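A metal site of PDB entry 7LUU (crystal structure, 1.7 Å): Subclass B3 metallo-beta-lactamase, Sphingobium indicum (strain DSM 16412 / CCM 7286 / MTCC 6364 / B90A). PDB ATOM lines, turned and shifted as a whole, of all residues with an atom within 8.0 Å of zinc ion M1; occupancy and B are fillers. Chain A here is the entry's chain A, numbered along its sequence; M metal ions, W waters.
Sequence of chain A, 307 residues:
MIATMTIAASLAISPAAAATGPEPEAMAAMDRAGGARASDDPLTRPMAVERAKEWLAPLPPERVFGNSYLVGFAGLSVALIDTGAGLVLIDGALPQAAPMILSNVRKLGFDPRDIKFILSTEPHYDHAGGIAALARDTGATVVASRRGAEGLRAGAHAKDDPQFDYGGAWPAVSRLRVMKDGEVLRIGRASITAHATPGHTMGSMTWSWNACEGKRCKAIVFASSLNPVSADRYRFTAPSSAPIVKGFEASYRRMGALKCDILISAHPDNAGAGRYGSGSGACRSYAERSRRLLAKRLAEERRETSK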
ATOM      1  N   THR A 121     -23.403  10.918  21.434  1.00  0.00           N
ATOM      2  CA  THR A 121     -23.936  12.275  21.406  1.00  0.00           C
ATOM      3  C   THR A 121     -25.381  12.323  20.935  1.00  0.00           C
ATOM      4  O   THR A 121     -26.097  13.301  21.253  1.00  0.00           O
ATOM      5  CB  THR A 121     -23.087  13.208  20.496  1.00  0.00           C
ATOM      6  OG1 THR A 121     -23.017  12.730  19.141  1.00  0.00           O
ATOM      7  CG2 THR A 121     -21.644  13.413  21.086  1.00  0.00           C
ATOM      8  N   GLU A 122     -25.779  11.378  20.072  1.00  0.00           N
ATOM      9  CA  GLU A 122     -27.135  11.398  19.497  1.00  0.00           C
ATOM     10  C   GLU A 122     -27.482  10.086  18.806  1.00  0.00           C
ATOM     11  O   GLU A 122     -26.602   9.407  18.237  1.00  0.00           O
ATOM     12  CB  GLU A 122     -27.321  12.543  18.484  1.00  0.00           C
ATOM     13  CG  GLU A 122     -26.331  12.405  17.249  1.00  0.00           C
ATOM     14  CD  GLU A 122     -26.684  13.382  16.134  1.00  0.00           C
ATOM     15  OE1 GLU A 122     -26.087  14.498  16.128  1.00  0.00           O
ATOM     16  OE2 GLU A 122     -27.481  13.035  15.257  1.00  0.00           O
ATOM     17  N   PRO A 123     -28.760   9.738  18.764  1.00  0.00           N
ATOM     18  CA  PRO A 123     -29.172   8.429  18.250  1.00  0.00           C
ATOM     19  C   PRO A 123     -29.574   8.515  16.772  1.00  0.00           C
ATOM     20  O   PRO A 123     -30.701   8.224  16.382  1.00  0.00           O
ATOM     21  CB  PRO A 123     -30.340   8.062  19.183  1.00  0.00           C
ATOM     22  CG  PRO A 123     -30.993   9.382  19.394  1.00  0.00           C
ATOM     23  CD  PRO A 123     -29.883  10.427  19.480  1.00  0.00           C
ATOM     24  N   HIS A 124     -28.636   9.000  15.927  1.00  0.00           N
ATOM     25  CA  HIS A 124     -28.818   9.014  14.493  1.00  0.00           C
ATOM     26  C   HIS A 124     -27.721   8.144  13.894  1.00  0.00           C
ATOM     27  O   HIS A 124     -26.641   7.970  14.503  1.00  0.00           O
ATOM     28  CB  HIS A 124     -28.674  10.421  13.949  1.00  0.00           C
ATOM     29  CG  HIS A 124     -29.891  11.265  14.136  1.00  0.00           C
ATOM     30  ND1 HIS A 124     -29.911  12.599  13.813  1.00  0.00           N
ATOM     31  CD2 HIS A 124     -31.147  10.943  14.557  1.00  0.00           C
ATOM     32  CE1 HIS A 124     -31.144  13.077  14.039  1.00  0.00           C
ATOM     33  NE2 HIS A 124     -31.909  12.095  14.481  1.00  0.00           N
ATOM     34  N   TYR A 125     -28.006   7.566  12.713  1.00  0.00           N
ATOM     35  CA  TYR A 125     -27.091   6.511  12.248  1.00  0.00           C
ATOM     36  C   TYR A 125     -25.692   7.009  11.848  1.00  0.00           C
ATOM     37  O   TYR A 125     -24.775   6.178  11.763  1.00  0.00           O
ATOM     38  CB  TYR A 125     -27.781   5.728  11.096  1.00  0.00           C
ATOM     39  CG  TYR A 125     -27.902   6.484   9.785  1.00  0.00           C
ATOM     40  CD1 TYR A 125     -26.788   6.683   8.990  1.00  0.00           C
ATOM     41  CD2 TYR A 125     -29.137   6.968   9.326  1.00  0.00           C
ATOM     42  CE1 TYR A 125     -26.864   7.315   7.790  1.00  0.00           C
ATOM     43  CE2 TYR A 125     -29.236   7.592   8.099  1.00  0.00           C
ATOM     44  CZ  TYR A 125     -28.084   7.786   7.357  1.00  0.00           C
ATOM     45  OH  TYR A 125     -28.155   8.419   6.133  1.00  0.00           O
ATOM     46  N   ASP A 126     -25.481   8.327  11.637  1.00  0.00           N
ATOM     47  CA  ASP A 126     -24.137   8.776  11.292  1.00  0.00           C
ATOM     48  C   ASP A 126     -23.287   8.997  12.532  1.00  0.00           C
ATOM     49  O   ASP A 126     -22.093   9.265  12.402  1.00  0.00           O
ATOM     50  CB  ASP A 126     -24.168  10.070  10.421  1.00  0.00           C
ATOM     51  CG  ASP A 126     -24.992  11.226  11.060  1.00  0.00           C
ATOM     52  OD1 ASP A 126     -26.041  10.979  11.702  1.00  0.00           O
ATOM     53  OD2 ASP A 126     -24.606  12.397  10.842  1.00  0.00           O
ATOM     54  N   HIS A 127     -23.842   8.850  13.755  1.00  0.00           N
ATOM     55  CA  HIS A 127     -23.051   8.904  14.976  1.00  0.00           C
ATOM     56  C   HIS A 127     -23.218   7.672  15.821  1.00  0.00           C
ATOM     57  O   HIS A 127     -22.299   7.295  16.531  1.00  0.00           O
ATOM     58  CB  HIS A 127     -23.435  10.153  15.831  1.00  0.00           C
ATOM     59  CG  HIS A 127     -23.471  11.410  15.012  1.00  0.00           C
ATOM     60  ND1 HIS A 127     -22.326  12.155  14.781  1.00  0.00           N
ATOM     61  CD2 HIS A 127     -24.453  11.979  14.280  1.00  0.00           C
ATOM     62  CE1 HIS A 127     -22.614  13.150  13.941  1.00  0.00           C
ATOM     63  NE2 HIS A 127     -23.898  13.066  13.637  1.00  0.00           N
ATOM     64  N   HIS A 157     -35.874   6.549  14.495  1.00  0.00           N
ATOM     65  CA  HIS A 157     -36.235   7.898  14.948  1.00  0.00           C
ATOM     66  C   HIS A 157     -37.391   7.897  15.930  1.00  0.00           C
ATOM     67  O   HIS A 157     -38.445   7.283  15.693  1.00  0.00           O
ATOM     68  CB  HIS A 157     -36.691   8.796  13.749  1.00  0.00           C
ATOM     69  CG  HIS A 157     -35.612   9.057  12.719  1.00  0.00           C
ATOM     70  ND1 HIS A 157     -34.585   9.957  12.924  1.00  0.00           N
ATOM     71  CD2 HIS A 157     -35.410   8.517  11.503  1.00  0.00           C
ATOM     72  CE1 HIS A 157     -33.822  10.011  11.830  1.00  0.00           C
ATOM     73  NE2 HIS A 157     -34.305   9.154  10.951  1.00  0.00           N
ATOM     74  N   ASP A 161     -38.483  13.537  17.024  1.00  0.00           N
ATOM     75  CA  ASP A 161     -37.243  13.880  16.338  1.00  0.00           C
ATOM     76  C   ASP A 161     -37.602  14.700  15.113  1.00  0.00           C
ATOM     77  O   ASP A 161     -38.501  14.303  14.364  1.00  0.00           O
ATOM     78  CB  ASP A 161     -36.568  12.557  15.952  1.00  0.00           C
ATOM     79  CG  ASP A 161     -35.216  12.708  15.308  1.00  0.00           C
ATOM     80  OD1 ASP A 161     -34.925  13.697  14.631  1.00  0.00           O
ATOM     81  OD2 ASP A 161     -34.441  11.756  15.475  1.00  0.00           O
ATOM     82  N   GLN A 163     -36.241  14.761  12.425  1.00  0.00           N
ATOM     83  CA  GLN A 163     -35.998  13.961  11.237  1.00  0.00           C
ATOM     84  C   GLN A 163     -36.816  12.669  11.249  1.00  0.00           C
ATOM     85  O   GLN A 163     -36.547  11.778  10.442  1.00  0.00           O
ATOM     86  CB  GLN A 163     -34.506  13.641  11.082  1.00  0.00           C
ATOM     87  CG  GLN A 163     -33.682  14.902  10.818  1.00  0.00           C
ATOM     88  CD  GLN A 163     -32.226  14.632  10.633  1.00  0.00           C
ATOM     89  OE1 GLN A 163     -31.354  15.138  11.390  1.00  0.00           O
ATOM     90  NE2 GLN A 163     -31.928  13.860   9.608  1.00  0.00           N
ATOM     91  N   HIS A 200     -31.024  19.373  18.176  1.00  0.00           N
ATOM     92  CA  HIS A 200     -30.952  18.538  16.976  1.00  0.00           C
ATOM     93  C   HIS A 200     -31.842  17.310  17.156  1.00  0.00           C
ATOM     94  O   HIS A 200     -32.598  16.914  16.238  1.00  0.00           O
ATOM     95  CB  HIS A 200     -29.477  18.175  16.753  1.00  0.00           C
ATOM     96  CG  HIS A 200     -29.242  17.296  15.565  1.00  0.00           C
ATOM     97  ND1 HIS A 200     -29.295  17.755  14.262  1.00  0.00           N
ATOM     98  CD2 HIS A 200     -28.966  15.967  15.504  1.00  0.00           C
ATOM     99  CE1 HIS A 200     -29.078  16.733  13.431  1.00  0.00           C
ATOM    100  NE2 HIS A 200     -28.851  15.648  14.164  1.00  0.00           N
ATOM    101  N   THR A 201     -31.758  16.713  18.350  1.00  0.00           N
ATOM    102  CA  THR A 201     -32.748  15.759  18.860  1.00  0.00           C
ATOM    103  C   THR A 201     -32.951  16.077  20.320  1.00  0.00           C
ATOM    104  O   THR A 201     -32.167  16.808  20.922  1.00  0.00           O
ATOM    105  CB  THR A 201     -32.306  14.295  18.726  1.00  0.00           C
ATOM    106  OG1 THR A 201     -31.231  14.011  19.644  1.00  0.00           O
ATOM    107  CG2 THR A 201     -31.833  13.941  17.303  1.00  0.00           C
ATOM    108  N   SER A 204     -29.883  14.721  22.504  1.00  0.00           N
ATOM    109  CA  SER A 204     -28.498  15.046  22.160  1.00  0.00           C
ATOM    110  C   SER A 204     -27.710  15.437  23.399  1.00  0.00           C
ATOM    111  O   SER A 204     -28.218  16.159  24.287  1.00  0.00           O
ATOM    112  CB  SER A 204     -28.479  16.202  21.138  1.00  0.00           C
ATOM    113  OG  SER A 204     -28.993  15.733  19.861  1.00  0.00           O
ATOM    114  N   SER A 225     -23.847  17.658  17.677  1.00  0.00           N
ATOM    115  CA  SER A 225     -24.445  18.553  16.694  1.00  0.00           C
ATOM    116  C   SER A 225     -25.490  19.443  17.341  1.00  0.00           C
ATOM    117  O   SER A 225     -26.311  18.976  18.120  1.00  0.00           O
ATOM    118  CB  SER A 225     -25.056  17.748  15.583  1.00  0.00           C
ATOM    119  OG  SER A 225     -25.687  18.637  14.637  1.00  0.00           O
ATOM    120  N   ASN A 227     -27.218  21.295  14.876  1.00  0.00           N
ATOM    121  CA  ASN A 227     -27.709  21.807  13.580  1.00  0.00           C
ATOM    122  C   ASN A 227     -29.219  21.670  13.531  1.00  0.00           C
ATOM    123  O   ASN A 227     -29.740  20.573  13.719  1.00  0.00           O
ATOM    124  CB  ASN A 227     -27.083  21.044  12.431  1.00  0.00           C
ATOM    125  CG  ASN A 227     -25.639  21.278  12.380  1.00  0.00           C
ATOM    126  OD1 ASN A 227     -25.165  22.391  12.700  1.00  0.00           O
ATOM    127  ND2 ASN A 227     -24.897  20.256  11.992  1.00  0.00           N
ATOM    128  N   VAL A 229     -31.843  20.828  11.678  1.00  0.00           N
ATOM    129  CA  VAL A 229     -32.273  20.238  10.416  1.00  0.00           C
ATOM    130  C   VAL A 229     -33.419  19.284  10.686  1.00  0.00           C
ATOM    131  O   VAL A 229     -33.648  18.819  11.812  1.00  0.00           O
ATOM    132  CB  VAL A 229     -31.115  19.551   9.693  1.00  0.00           C
ATOM    133  CG1 VAL A 229     -30.151  20.612   9.238  1.00  0.00           C
ATOM    134  CG2 VAL A 229     -30.471  18.599  10.607  1.00  0.00           C
ATOM    135  N   HIS A 267     -19.768  16.658  13.837  1.00  0.00           N
ATOM    136  CA  HIS A 267     -19.324  16.893  12.464  1.00  0.00           C
ATOM    137  C   HIS A 267     -18.201  17.927  12.528  1.00  0.00           C
ATOM    138  O   HIS A 267     -18.498  19.094  12.825  1.00  0.00           O
ATOM    139  CB  HIS A 267     -20.499  17.478  11.643  1.00  0.00           C
ATOM    140  CG  HIS A 267     -21.585  16.463  11.382  1.00  0.00           C
ATOM    141  ND1 HIS A 267     -21.545  15.623  10.283  1.00  0.00           N
ATOM    142  CD2 HIS A 267     -22.690  16.133  12.079  1.00  0.00           C
ATOM    143  CE1 HIS A 267     -22.599  14.846  10.305  1.00  0.00           C
ATOM    144  NE2 HIS A 267     -23.303  15.098  11.407  1.00  0.00           N
HETATM  145 ZN    ZN M   1     -28.269  13.791  13.688  1.00  0.00          ZN
HETATM  146 ZN    ZN M   2     -24.866  14.016  12.138  1.00  0.00          ZN
HETATM  147  O   HOH W   1     -27.004  13.322  12.296  1.00  0.00           O
HETATM  148  O   HOH W   2     -25.498  15.580  13.338  1.00  0.00           O
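O of Asn 227 is in hydrogen-bond range of ND1 of His 200 (2.9 Å).
NE2 of His 124 lies within hydrogen-bond range of OD2 of Asp 161, 2.7 Å away.
Water W2 bridges the side-chain carboxylate of Glu 122 (3.0 Å) and the side-chain hydroxyl of Ser 225 (3.3 Å).
Within 4 Å of zinc ion M1: Glu 122, His 124 and His 200.
The nearest printed residue that does not touch zinc ion M1 is Gln 163 (4.1 Å).
The side-chain carboxylate (OE2) of Glu 122 binds zinc ion M1 (1.9 Å).
Water W1 is bound to zinc ion M1 (1.9 Å).
NE2 of His 200 is bound to zinc ion M1, at 2.0 Å.
A ring nitrogen (ND1) of His 124 binds zinc ion M1 (2.0 Å).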
